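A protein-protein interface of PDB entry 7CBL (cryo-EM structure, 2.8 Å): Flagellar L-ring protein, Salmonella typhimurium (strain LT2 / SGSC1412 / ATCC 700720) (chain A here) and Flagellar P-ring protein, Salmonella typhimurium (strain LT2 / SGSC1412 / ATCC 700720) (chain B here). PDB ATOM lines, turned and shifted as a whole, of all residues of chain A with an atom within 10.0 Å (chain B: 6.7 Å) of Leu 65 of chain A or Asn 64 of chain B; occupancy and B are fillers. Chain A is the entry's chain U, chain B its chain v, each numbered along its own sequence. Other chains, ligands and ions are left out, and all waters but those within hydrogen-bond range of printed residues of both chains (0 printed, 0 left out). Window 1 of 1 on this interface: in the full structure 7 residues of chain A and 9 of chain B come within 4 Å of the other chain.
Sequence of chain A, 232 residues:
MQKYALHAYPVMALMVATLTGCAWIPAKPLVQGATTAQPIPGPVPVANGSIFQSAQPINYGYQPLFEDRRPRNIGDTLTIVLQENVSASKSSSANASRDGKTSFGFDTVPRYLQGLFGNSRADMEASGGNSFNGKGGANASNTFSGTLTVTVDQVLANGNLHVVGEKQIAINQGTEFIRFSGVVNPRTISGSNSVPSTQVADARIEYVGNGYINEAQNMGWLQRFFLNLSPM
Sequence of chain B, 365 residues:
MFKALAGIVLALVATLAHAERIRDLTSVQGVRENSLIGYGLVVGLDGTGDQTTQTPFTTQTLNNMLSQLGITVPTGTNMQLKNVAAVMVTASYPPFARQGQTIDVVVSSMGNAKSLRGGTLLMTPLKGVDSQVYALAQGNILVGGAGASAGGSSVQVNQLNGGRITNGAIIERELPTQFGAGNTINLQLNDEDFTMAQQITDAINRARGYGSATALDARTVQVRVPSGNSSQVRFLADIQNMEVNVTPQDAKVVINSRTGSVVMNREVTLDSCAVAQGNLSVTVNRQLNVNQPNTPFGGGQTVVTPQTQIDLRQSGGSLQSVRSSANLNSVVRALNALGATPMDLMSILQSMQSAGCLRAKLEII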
ATOM      1  N   GLY A  61     -16.922 -15.006  -1.390  1.00  0.00           N
ATOM      2  CA  GLY A  61     -18.251 -14.948  -1.949  1.00  0.00           C
ATOM      3  C   GLY A  61     -19.188 -15.986  -1.357  1.00  0.00           C
ATOM      4  O   GLY A  61     -18.880 -16.706  -0.407  1.00  0.00           O
ATOM      5  N   TYR A  62     -20.375 -16.044  -1.950  1.00  0.00           N
ATOM      6  CA  TYR A  62     -21.366 -17.032  -1.558  1.00  0.00           C
ATOM      7  C   TYR A  62     -20.836 -18.433  -1.812  1.00  0.00           C
ATOM      8  O   TYR A  62     -20.274 -18.713  -2.872  1.00  0.00           O
ATOM      9  CB  TYR A  62     -22.657 -16.798  -2.335  1.00  0.00           C
ATOM     10  CG  TYR A  62     -23.539 -18.012  -2.455  1.00  0.00           C
ATOM     11  CD1 TYR A  62     -24.310 -18.435  -1.389  1.00  0.00           C
ATOM     12  CD2 TYR A  62     -23.608 -18.728  -3.635  1.00  0.00           C
ATOM     13  CE1 TYR A  62     -25.117 -19.539  -1.491  1.00  0.00           C
ATOM     14  CE2 TYR A  62     -24.412 -19.834  -3.746  1.00  0.00           C
ATOM     15  CZ  TYR A  62     -25.165 -20.234  -2.669  1.00  0.00           C
ATOM     16  OH  TYR A  62     -25.971 -21.336  -2.770  1.00  0.00           O
ATOM     17  N   GLN A  63     -21.009 -19.316  -0.833  1.00  0.00           N
ATOM     18  CA  GLN A  63     -20.523 -20.686  -0.926  1.00  0.00           C
ATOM     19  C   GLN A  63     -21.675 -21.634  -0.622  1.00  0.00           C
ATOM     20  O   GLN A  63     -22.263 -21.556   0.473  1.00  0.00           O
ATOM     21  CB  GLN A  63     -19.358 -20.917   0.033  1.00  0.00           C
ATOM     22  CG  GLN A  63     -18.171 -20.020  -0.236  1.00  0.00           C
ATOM     23  CD  GLN A  63     -17.318 -19.808   0.990  1.00  0.00           C
ATOM     24  OE1 GLN A  63     -16.956 -18.680   1.320  1.00  0.00           O
ATOM     25  NE2 GLN A  63     -16.987 -20.894   1.673  1.00  0.00           N
ATOM     26  N   PRO A  64     -22.028 -22.533  -1.537  1.00  0.00           N
ATOM     27  CA  PRO A  64     -23.139 -23.456  -1.285  1.00  0.00           C
ATOM     28  C   PRO A  64     -22.840 -24.376  -0.115  1.00  0.00           C
ATOM     29  O   PRO A  64     -21.717 -24.462   0.381  1.00  0.00           O
ATOM     30  CB  PRO A  64     -23.256 -24.237  -2.595  1.00  0.00           C
ATOM     31  CG  PRO A  64     -22.552 -23.409  -3.602  1.00  0.00           C
ATOM     32  CD  PRO A  64     -21.455 -22.716  -2.876  1.00  0.00           C
ATOM     33  N   LEU A  65     -23.872 -25.087   0.322  1.00  0.00           N
ATOM     34  CA  LEU A  65     -23.785 -25.928   1.506  1.00  0.00           C
ATOM     35  C   LEU A  65     -23.761 -27.412   1.183  1.00  0.00           C
ATOM     36  O   LEU A  65     -22.928 -28.144   1.718  1.00  0.00           O
ATOM     37  CB  LEU A  65     -24.957 -25.620   2.442  1.00  0.00           C
ATOM     38  CG  LEU A  65     -24.636 -25.514   3.929  1.00  0.00           C
ATOM     39  CD1 LEU A  65     -23.701 -24.359   4.185  1.00  0.00           C
ATOM     40  CD2 LEU A  65     -25.913 -25.349   4.720  1.00  0.00           C
ATOM     41  N   PHE A  66     -24.656 -27.882   0.319  1.00  0.00           N
ATOM     42  CA  PHE A  66     -24.757 -29.301   0.020  1.00  0.00           C
ATOM     43  C   PHE A  66     -24.059 -29.696  -1.270  1.00  0.00           C
ATOM     44  O   PHE A  66     -23.833 -30.887  -1.491  1.00  0.00           O
ATOM     45  CB  PHE A  66     -26.226 -29.720  -0.051  1.00  0.00           C
ATOM     46  CG  PHE A  66     -27.037 -29.258   1.115  1.00  0.00           C
ATOM     47  CD1 PHE A  66     -26.859 -29.821   2.360  1.00  0.00           C
ATOM     48  CD2 PHE A  66     -27.965 -28.253   0.970  1.00  0.00           C
ATOM     49  CE1 PHE A  66     -27.594 -29.393   3.432  1.00  0.00           C
ATOM     50  CE2 PHE A  66     -28.703 -27.823   2.042  1.00  0.00           C
ATOM     51  CZ  PHE A  66     -28.517 -28.393   3.274  1.00  0.00           C
ATOM     52  N   GLU A  67     -23.716 -28.738  -2.120  1.00  0.00           N
ATOM     53  CA  GLU A  67     -23.048 -29.060  -3.367  1.00  0.00           C
ATOM     54  C   GLU A  67     -21.613 -29.496  -3.109  1.00  0.00           C
ATOM     55  O   GLU A  67     -20.955 -29.030  -2.176  1.00  0.00           O
ATOM     56  CB  GLU A  67     -23.073 -27.858  -4.301  1.00  0.00           C
ATOM     57  CG  GLU A  67     -24.451 -27.270  -4.468  1.00  0.00           C
ATOM     58  CD  GLU A  67     -24.487 -26.155  -5.481  1.00  0.00           C
ATOM     59  OE1 GLU A  67     -23.696 -26.203  -6.444  1.00  0.00           O
ATOM     60  OE2 GLU A  67     -25.310 -25.230  -5.320  1.00  0.00           O
ATOM     61  N   ASP A  68     -21.130 -30.402  -3.954  1.00  0.00           N
ATOM     62  CA  ASP A  68     -19.765 -30.884  -3.834  1.00  0.00           C
ATOM     63  C   ASP A  68     -18.778 -29.746  -4.060  1.00  0.00           C
ATOM     64  O   ASP A  68     -19.090 -28.733  -4.687  1.00  0.00           O
ATOM     65  CB  ASP A  68     -19.503 -32.001  -4.838  1.00  0.00           C
ATOM     66  CG  ASP A  68     -20.274 -33.258  -4.524  1.00  0.00           C
ATOM     67  OD1 ASP A  68     -19.879 -33.987  -3.599  1.00  0.00           O
ATOM     68  OD2 ASP A  68     -21.280 -33.518  -5.205  1.00  0.00           O
ATOM     69  N   ARG A  69     -17.570 -29.924  -3.539  1.00  0.00           N
ATOM     70  CA  ARG A  69     -16.526 -28.914  -3.688  1.00  0.00           C
ATOM     71  C   ARG A  69     -15.912 -29.056  -5.072  1.00  0.00           C
ATOM     72  O   ARG A  69     -14.916 -29.748  -5.271  1.00  0.00           O
ATOM     73  CB  ARG A  69     -15.479 -29.050  -2.593  1.00  0.00           C
ATOM     74  CG  ARG A  69     -15.162 -30.470  -2.196  1.00  0.00           C
ATOM     75  CD  ARG A  69     -14.255 -30.489  -0.988  1.00  0.00           C
ATOM     76  NE  ARG A  69     -13.758 -31.826  -0.701  1.00  0.00           N
ATOM     77  CZ  ARG A  69     -12.525 -32.232  -0.973  1.00  0.00           C
ATOM     78  NH1 ARG A  69     -11.666 -31.400  -1.541  1.00  0.00           N
ATOM     79  NH2 ARG A  69     -12.152 -33.467  -0.676  1.00  0.00           N
ATOM     80  N   ARG A  70     -16.503 -28.425  -6.006  1.00  0.00           N
ATOM     81  CA  ARG A  70     -15.922 -28.378  -7.329  1.00  0.00           C
ATOM     82  C   ARG A  70     -15.171 -27.070  -7.523  1.00  0.00           C
ATOM     83  O   ARG A  70     -15.518 -26.056  -6.916  1.00  0.00           O
ATOM     84  CB  ARG A  70     -17.001 -28.490  -8.405  1.00  0.00           C
ATOM     85  CG  ARG A  70     -17.698 -29.822  -8.458  1.00  0.00           C
ATOM     86  CD  ARG A  70     -18.879 -29.752  -9.393  1.00  0.00           C
ATOM     87  NE  ARG A  70     -19.563 -31.031  -9.509  1.00  0.00           N
ATOM     88  CZ  ARG A  70     -20.670 -31.216 -10.216  1.00  0.00           C
ATOM     89  NH1 ARG A  70     -21.216 -30.202 -10.868  1.00  0.00           N
ATOM     90  NH2 ARG A  70     -21.231 -32.413 -10.271  1.00  0.00           N
ATOM     91  N   ARG A  72     -14.500 -23.667  -9.259  1.00  0.00           N
ATOM     92  CA  ARG A  72     -15.416 -22.767  -9.946  1.00  0.00           C
ATOM     93  C   ARG A  72     -14.770 -21.518 -10.513  1.00  0.00           C
ATOM     94  O   ARG A  72     -15.320 -20.950 -11.461  1.00  0.00           O
ATOM     95  CB  ARG A  72     -16.551 -22.338  -9.009  1.00  0.00           C
ATOM     96  CG  ARG A  72     -17.340 -23.488  -8.433  1.00  0.00           C
ATOM     97  CD  ARG A  72     -18.398 -23.000  -7.470  1.00  0.00           C
ATOM     98  NE  ARG A  72     -18.578 -23.927  -6.360  1.00  0.00           N
ATOM     99  CZ  ARG A  72     -19.410 -24.960  -6.380  1.00  0.00           C
ATOM    100  NH1 ARG A  72     -20.144 -25.201  -7.455  1.00  0.00           N
ATOM    101  NH2 ARG A  72     -19.510 -25.754  -5.324  1.00  0.00           N
ATOM    102  N   SER A 190     -15.636 -35.977  -9.439  1.00  0.00           N
ATOM    103  CA  SER A 190     -16.265 -36.856  -8.469  1.00  0.00           C
ATOM    104  C   SER A 190     -16.556 -36.100  -7.177  1.00  0.00           C
ATOM    105  O   SER A 190     -16.299 -34.902  -7.047  1.00  0.00           O
ATOM    106  CB  SER A 190     -15.379 -38.067  -8.201  1.00  0.00           C
ATOM    107  OG  SER A 190     -14.391 -37.763  -7.239  1.00  0.00           O
ATOM    108  N   GLY A 191     -17.105 -36.824  -6.201  1.00  0.00           N
ATOM    109  CA  GLY A 191     -17.437 -36.222  -4.924  1.00  0.00           C
ATOM    110  C   GLY A 191     -16.236 -35.835  -4.093  1.00  0.00           C
ATOM    111  O   GLY A 191     -16.360 -34.995  -3.196  1.00  0.00           O
ATOM    112  N   SER A 192     -15.075 -36.427  -4.367  1.00  0.00           N
ATOM    113  CA  SER A 192     -13.849 -36.125  -3.646  1.00  0.00           C
ATOM    114  C   SER A 192     -12.943 -35.173  -4.413  1.00  0.00           C
ATOM    115  O   SER A 192     -11.738 -35.133  -4.152  1.00  0.00           O
ATOM    116  CB  SER A 192     -13.101 -37.414  -3.317  1.00  0.00           C
ATOM    117  OG  SER A 192     -13.032 -38.258  -4.450  1.00  0.00           O
ATOM    118  N   ASN A 193     -13.499 -34.413  -5.356  1.00  0.00           N
ATOM    119  CA  ASN A 193     -12.761 -33.413  -6.122  1.00  0.00           C
ATOM    120  C   ASN A 193     -11.619 -34.053  -6.909  1.00  0.00           C
ATOM    121  O   ASN A 193     -10.455 -33.679  -6.786  1.00  0.00           O
ATOM    122  CB  ASN A 193     -12.242 -32.305  -5.204  1.00  0.00           C
ATOM    123  CG  ASN A 193     -11.943 -31.035  -5.947  1.00  0.00           C
ATOM    124  OD1 ASN A 193     -12.566 -30.737  -6.959  1.00  0.00           O
ATOM    125  ND2 ASN A 193     -10.986 -30.270  -5.448  1.00  0.00           N
ATOM    126  N   THR B  59     -26.130 -38.605   3.353  1.00  0.00           N
ATOM    127  CA  THR B  59     -24.903 -38.501   4.132  1.00  0.00           C
ATOM    128  C   THR B  59     -23.845 -37.698   3.395  1.00  0.00           C
ATOM    129  O   THR B  59     -23.073 -36.963   4.017  1.00  0.00           O
ATOM    130  CB  THR B  59     -24.365 -39.888   4.467  1.00  0.00           C
ATOM    131  OG1 THR B  59     -24.258 -40.658   3.265  1.00  0.00           O
ATOM    132  CG2 THR B  59     -25.281 -40.591   5.433  1.00  0.00           C
ATOM    133  N   GLN B  60     -23.795 -37.816   2.068  1.00  0.00           N
ATOM    134  CA  GLN B  60     -22.794 -37.071   1.314  1.00  0.00           C
ATOM    135  C   GLN B  60     -23.015 -35.571   1.439  1.00  0.00           C
ATOM    136  O   GLN B  60     -22.071 -34.808   1.674  1.00  0.00           O
ATOM    137  CB  GLN B  60     -22.816 -37.499  -0.148  1.00  0.00           C
ATOM    138  CG  GLN B  60     -21.921 -36.665  -1.027  1.00  0.00           C
ATOM    139  CD  GLN B  60     -21.750 -37.261  -2.396  1.00  0.00           C
ATOM    140  OE1 GLN B  60     -22.004 -38.445  -2.603  1.00  0.00           O
ATOM    141  NE2 GLN B  60     -21.315 -36.446  -3.345  1.00  0.00           N
ATOM    142  N   THR B  61     -24.261 -35.124   1.295  1.00  0.00           N
ATOM    143  CA  THR B  61     -24.543 -33.701   1.413  1.00  0.00           C
ATOM    144  C   THR B  61     -24.407 -33.216   2.848  1.00  0.00           C
ATOM    145  O   THR B  61     -24.010 -32.069   3.077  1.00  0.00           O
ATOM    146  CB  THR B  61     -25.934 -33.410   0.875  1.00  0.00           C
ATOM    147  OG1 THR B  61     -26.837 -34.417   1.340  1.00  0.00           O
ATOM    148  CG2 THR B  61     -25.915 -33.442  -0.629  1.00  0.00           C
ATOM    149  N   LEU B  62     -24.713 -34.069   3.826  1.00  0.00           N
ATOM    150  CA  LEU B  62     -24.456 -33.692   5.209  1.00  0.00           C
ATOM    151  C   LEU B  62     -22.968 -33.484   5.453  1.00  0.00           C
ATOM    152  O   LEU B  62     -22.569 -32.539   6.142  1.00  0.00           O
ATOM    153  CB  LEU B  62     -25.011 -34.750   6.155  1.00  0.00           C
ATOM    154  CG  LEU B  62     -25.014 -34.341   7.624  1.00  0.00           C
ATOM    155  CD1 LEU B  62     -26.327 -33.692   7.992  1.00  0.00           C
ATOM    156  CD2 LEU B  62     -24.747 -35.536   8.503  1.00  0.00           C
ATOM    157  N   ASN B  63     -22.129 -34.356   4.890  1.00  0.00           N
ATOM    158  CA  ASN B  63     -20.689 -34.176   5.012  1.00  0.00           C
ATOM    159  C   ASN B  63     -20.232 -32.907   4.312  1.00  0.00           C
ATOM    160  O   ASN B  63     -19.348 -32.204   4.807  1.00  0.00           O
ATOM    161  CB  ASN B  63     -19.953 -35.382   4.445  1.00  0.00           C
ATOM    162  CG  ASN B  63     -20.029 -36.581   5.348  1.00  0.00           C
ATOM    163  OD1 ASN B  63     -20.356 -36.462   6.526  1.00  0.00           O
ATOM    164  ND2 ASN B  63     -19.722 -37.749   4.806  1.00  0.00           N
ATOM    165  N   ASN B  64     -20.808 -32.606   3.150  1.00  0.00           N
ATOM    166  CA  ASN B  64     -20.474 -31.358   2.475  1.00  0.00           C
ATOM    167  C   ASN B  64     -20.792 -30.158   3.353  1.00  0.00           C
ATOM    168  O   ASN B  64     -19.985 -29.230   3.467  1.00  0.00           O
ATOM    169  CB  ASN B  64     -21.220 -31.251   1.151  1.00  0.00           C
ATOM    170  CG  ASN B  64     -20.744 -32.253   0.137  1.00  0.00           C
ATOM    171  OD1 ASN B  64     -19.731 -32.913   0.336  1.00  0.00           O
ATOM    172  ND2 ASN B  64     -21.472 -32.374  -0.961  1.00  0.00           N
ATOM    173  N   MET B  65     -21.962 -30.163   3.988  1.00  0.00           N
ATOM    174  CA  MET B  65     -22.338 -29.039   4.841  1.00  0.00           C
ATOM    175  C   MET B  65     -21.419 -28.930   6.048  1.00  0.00           C
ATOM    176  O   MET B  65     -20.974 -27.833   6.406  1.00  0.00           O
ATOM    177  CB  MET B  65     -23.788 -29.181   5.288  1.00  0.00           C
ATOM    178  CG  MET B  65     -24.232 -28.094   6.236  1.00  0.00           C
ATOM    179  SD  MET B  65     -25.804 -28.462   7.021  1.00  0.00           S
ATOM    180  CE  MET B  65     -25.446 -30.050   7.756  1.00  0.00           C
ATOM    181  N   LEU B  66     -21.125 -30.058   6.693  1.00  0.00           N
ATOM    182  CA  LEU B  66     -20.236 -30.035   7.849  1.00  0.00           C
ATOM    183  C   LEU B  66     -18.860 -29.513   7.468  1.00  0.00           C
ATOM    184  O   LEU B  66     -18.273 -28.698   8.185  1.00  0.00           O
ATOM    185  CB  LEU B  66     -20.128 -31.431   8.458  1.00  0.00           C
ATOM    186  CG  LEU B  66     -21.310 -31.907   9.296  1.00  0.00           C
ATOM    187  CD1 LEU B  66     -21.012 -33.267   9.879  1.00  0.00           C
ATOM    188  CD2 LEU B  66     -21.614 -30.913  10.390  1.00  0.00           C
ATOM    189  N   SER B  67     -18.329 -29.975   6.336  1.00  0.00           N
ATOM    190  CA  SER B  67     -17.037 -29.491   5.868  1.00  0.00           C
ATOM    191  C   SER B  67     -17.076 -27.998   5.592  1.00  0.00           C
ATOM    192  O   SER B  67     -16.135 -27.274   5.925  1.00  0.00           O
ATOM    193  CB  SER B  67     -16.622 -30.256   4.618  1.00  0.00           C
ATOM    194  OG  SER B  67     -15.446 -29.713   4.056  1.00  0.00           O
ATOM    195  N   GLN B  68     -18.159 -27.519   4.982  1.00  0.00           N
ATOM    196  CA  GLN B  68     -18.291 -26.090   4.738  1.00  0.00           C
ATOM    197  C   GLN B  68     -18.308 -25.301   6.037  1.00  0.00           C
ATOM    198  O   GLN B  68     -17.778 -24.187   6.094  1.00  0.00           O
ATOM    199  CB  GLN B  68     -19.558 -25.820   3.934  1.00  0.00           C
ATOM    200  CG  GLN B  68     -19.891 -24.362   3.782  1.00  0.00           C
ATOM    201  CD  GLN B  68     -18.777 -23.593   3.129  1.00  0.00           C
ATOM    202  OE1 GLN B  68     -18.230 -24.017   2.116  1.00  0.00           O
ATOM    203  NE2 GLN B  68     -18.427 -22.457   3.707  1.00  0.00           N
ATOM    204  N   LEU B  69     -18.902 -25.858   7.092  1.00  0.00           N
ATOM    205  CA  LEU B  69     -18.966 -25.150   8.364  1.00  0.00           C
ATOM    206  C   LEU B  69     -17.652 -25.184   9.130  1.00  0.00           C
ATOM    207  O   LEU B  69     -17.421 -24.308   9.967  1.00  0.00           O
ATOM    208  CB  LEU B  69     -20.079 -25.727   9.235  1.00  0.00           C
ATOM    209  CG  LEU B  69     -21.492 -25.336   8.811  1.00  0.00           C
ATOM    210  CD1 LEU B  69     -22.506 -26.058   9.656  1.00  0.00           C
ATOM    211  CD2 LEU B  69     -21.679 -23.841   8.917  1.00  0.00           C
ATOM    212  N   ILE B  71     -15.913 -28.550   9.908  1.00  0.00           N
ATOM    213  CA  ILE B  71     -15.723 -29.850  10.538  1.00  0.00           C
ATOM    214  C   ILE B  71     -15.563 -30.889   9.442  1.00  0.00           C
ATOM    215  O   ILE B  71     -16.478 -31.087   8.638  1.00  0.00           O
ATOM    216  CB  ILE B  71     -16.895 -30.220  11.457  1.00  0.00           C
ATOM    217  CG1 ILE B  71     -17.067 -29.165  12.544  1.00  0.00           C
ATOM    218  CG2 ILE B  71     -16.679 -31.585  12.064  1.00  0.00           C
ATOM    219  CD1 ILE B  71     -18.494 -28.894  12.891  1.00  0.00           C
ATOM    220  N   LEU B 122     -33.226 -26.429   6.137  1.00  0.00           N
ATOM    221  CA  LEU B 122     -31.980 -25.688   6.206  1.00  0.00           C
ATOM    222  C   LEU B 122     -31.788 -24.850   4.946  1.00  0.00           C
ATOM    223  O   LEU B 122     -32.515 -24.985   3.963  1.00  0.00           O
ATOM    224  CB  LEU B 122     -30.806 -26.638   6.398  1.00  0.00           C
ATOM    225  CG  LEU B 122     -30.843 -27.443   7.691  1.00  0.00           C
ATOM    226  CD1 LEU B 122     -29.650 -28.358   7.779  1.00  0.00           C
ATOM    227  CD2 LEU B 122     -30.880 -26.507   8.873  1.00  0.00           C
ATOM    228  N   MET B 123     -30.785 -23.980   4.985  1.00  0.00           N
ATOM    229  CA  MET B 123     -30.560 -23.013   3.918  1.00  0.00           C
ATOM    230  C   MET B 123     -30.432 -23.696   2.565  1.00  0.00           C
ATOM    231  O   MET B 123     -29.535 -24.512   2.351  1.00  0.00           O
ATOM    232  CB  MET B 123     -29.303 -22.205   4.217  1.00  0.00           C
ATOM    233  CG  MET B 123     -28.837 -21.381   3.050  1.00  0.00           C
ATOM    234  SD  MET B 123     -30.142 -20.297   2.471  1.00  0.00           S
ATOM    235  CE  MET B 123     -30.365 -19.281   3.916  1.00  0.00           C
ATOM    236  N   THR B 124     -31.328 -23.344   1.647  1.00  0.00           N
ATOM    237  CA  THR B 124     -31.423 -23.994   0.353  1.00  0.00           C
ATOM    238  C   THR B 124     -31.537 -22.938  -0.738  1.00  0.00           C
ATOM    239  O   THR B 124     -32.400 -22.051  -0.649  1.00  0.00           O
ATOM    240  CB  THR B 124     -32.637 -24.925   0.309  1.00  0.00           C
ATOM    241  OG1 THR B 124     -32.381 -26.083   1.107  1.00  0.00           O
ATOM    242  CG2 THR B 124     -32.930 -25.350  -1.106  1.00  0.00           C
ATOM    243  N   PRO B 125     -30.695 -22.985  -1.768  1.00  0.00           N
ATOM    244  CA  PRO B 125     -30.857 -22.073  -2.903  1.00  0.00           C
ATOM    245  C   PRO B 125     -31.787 -22.648  -3.958  1.00  0.00           C
ATOM    246  O   PRO B 125     -31.749 -23.837  -4.278  1.00  0.00           O
ATOM    247  CB  PRO B 125     -29.427 -21.954  -3.440  1.00  0.00           C
ATOM    248  CG  PRO B 125     -28.830 -23.271  -3.143  1.00  0.00           C
ATOM    249  CD  PRO B 125     -29.472 -23.792  -1.886  1.00  0.00           C
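NE2 of Gln 63 of chain A sits close to NE2 of Gln 68 of chain B (2.9 Å). N of Met 65 of chain B lies within hydrogen-bond range of O of Leu 65 of chain A, at 3.2 Å. The backbone carbonyl oxygen (O) of Phe 66 of chain A lies within hydrogen-bond range of the side-chain amide nitrogen (ND2) of Asn 64 of chain B (2.8 Å). OD1 of Asp 68 of chain A lies within hydrogen-bond range of NE2 of Gln 60 of chain B, 2.9 Å away. The side-chain carboxylate (OD1) of Asp 68 of chain A lies within hydrogen-bond range of the side-chain amide nitrogen (ND2) of Asn 64 of chain B.
OE1 of Gln 63 of chain A sits close to O of Gly 61 of chain A (3.3 Å). OE1 of Glu 67 of chain A is in salt-bridge range of NH1 of Arg 72 of chain A. O of Asp 68 of chain A lies within hydrogen-bond range of NH2 of Arg 72 of chain A (3.1 Å). O of Gln 60 of chain B sits close to OD1 of Asn 64 of chain B, at 3.3 Å.
Among the printed residues, pairs that only touch across the chains: Leu 65 of chain A with Asn 64 of chain B, Phe 66 of chain A with Thr 61 of chain B, Phe 66 of chain A with Met 123 of chain B, Tyr 62 of chain A with Pro 125 of chain B, Glu 67 of chain A with Asn 64 of chain B, Leu 65 of chain A with Gln 68 of chain B and Pro 64 of chain A with Gln 68 of chain B.
Of the printed residues of chain B, Tyr 62 of chain A touches Pro 125 (3.5 Å). Leu 65 of chain A touches three residues of chain B. Of the printed residues of chain B, Glu 67 of chain A touches Asn 64 (3.6 Å). Arg 69 of chain A touches none of the printed residues of chain B. Of the printed residues of chain A, Gln 60 of chain B touches Asp 68. No residue of chain A comes within 4 Å of Asn 63 of chain B. Asn 64 of chain B touches just these residues of chain A: Leu 65 (3.4 Å), Phe 66 (2.8 Å), Glu 67 (3.6 Å) and Asp 68 (3.5 Å). Printed residues of chain A within 4 Å of Pro 125 of chain B: Tyr 62. The nearest residue of chain B that does not touch Leu 65 of chain A is Thr 61 of chain B (4.3 Å).
Of the 15 printed residues of chain A, 7 touch a printed residue of chain B. Printed residues of chain A that touch a printed residue of chain B: Tyr 62, Gln 63, Pro 64, Leu 65, Phe 66, Glu 67 and Asp 68. Hydrophobic or aromatic side chains of chain A that line the printed part of chain B: Tyr 62, Leu 65 and Phe 66. Along chain A the printed residues that touch a printed residue of chain B span positions 62 to 68. Of the 16 printed residues of chain B, 7 touch a printed residue of chain A. Hydrophobic or aromatic side chains of chain B that line the printed part of chain A: Met 65 and Pro 125. Among the printed residues, 12 pairs touch across the chains.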
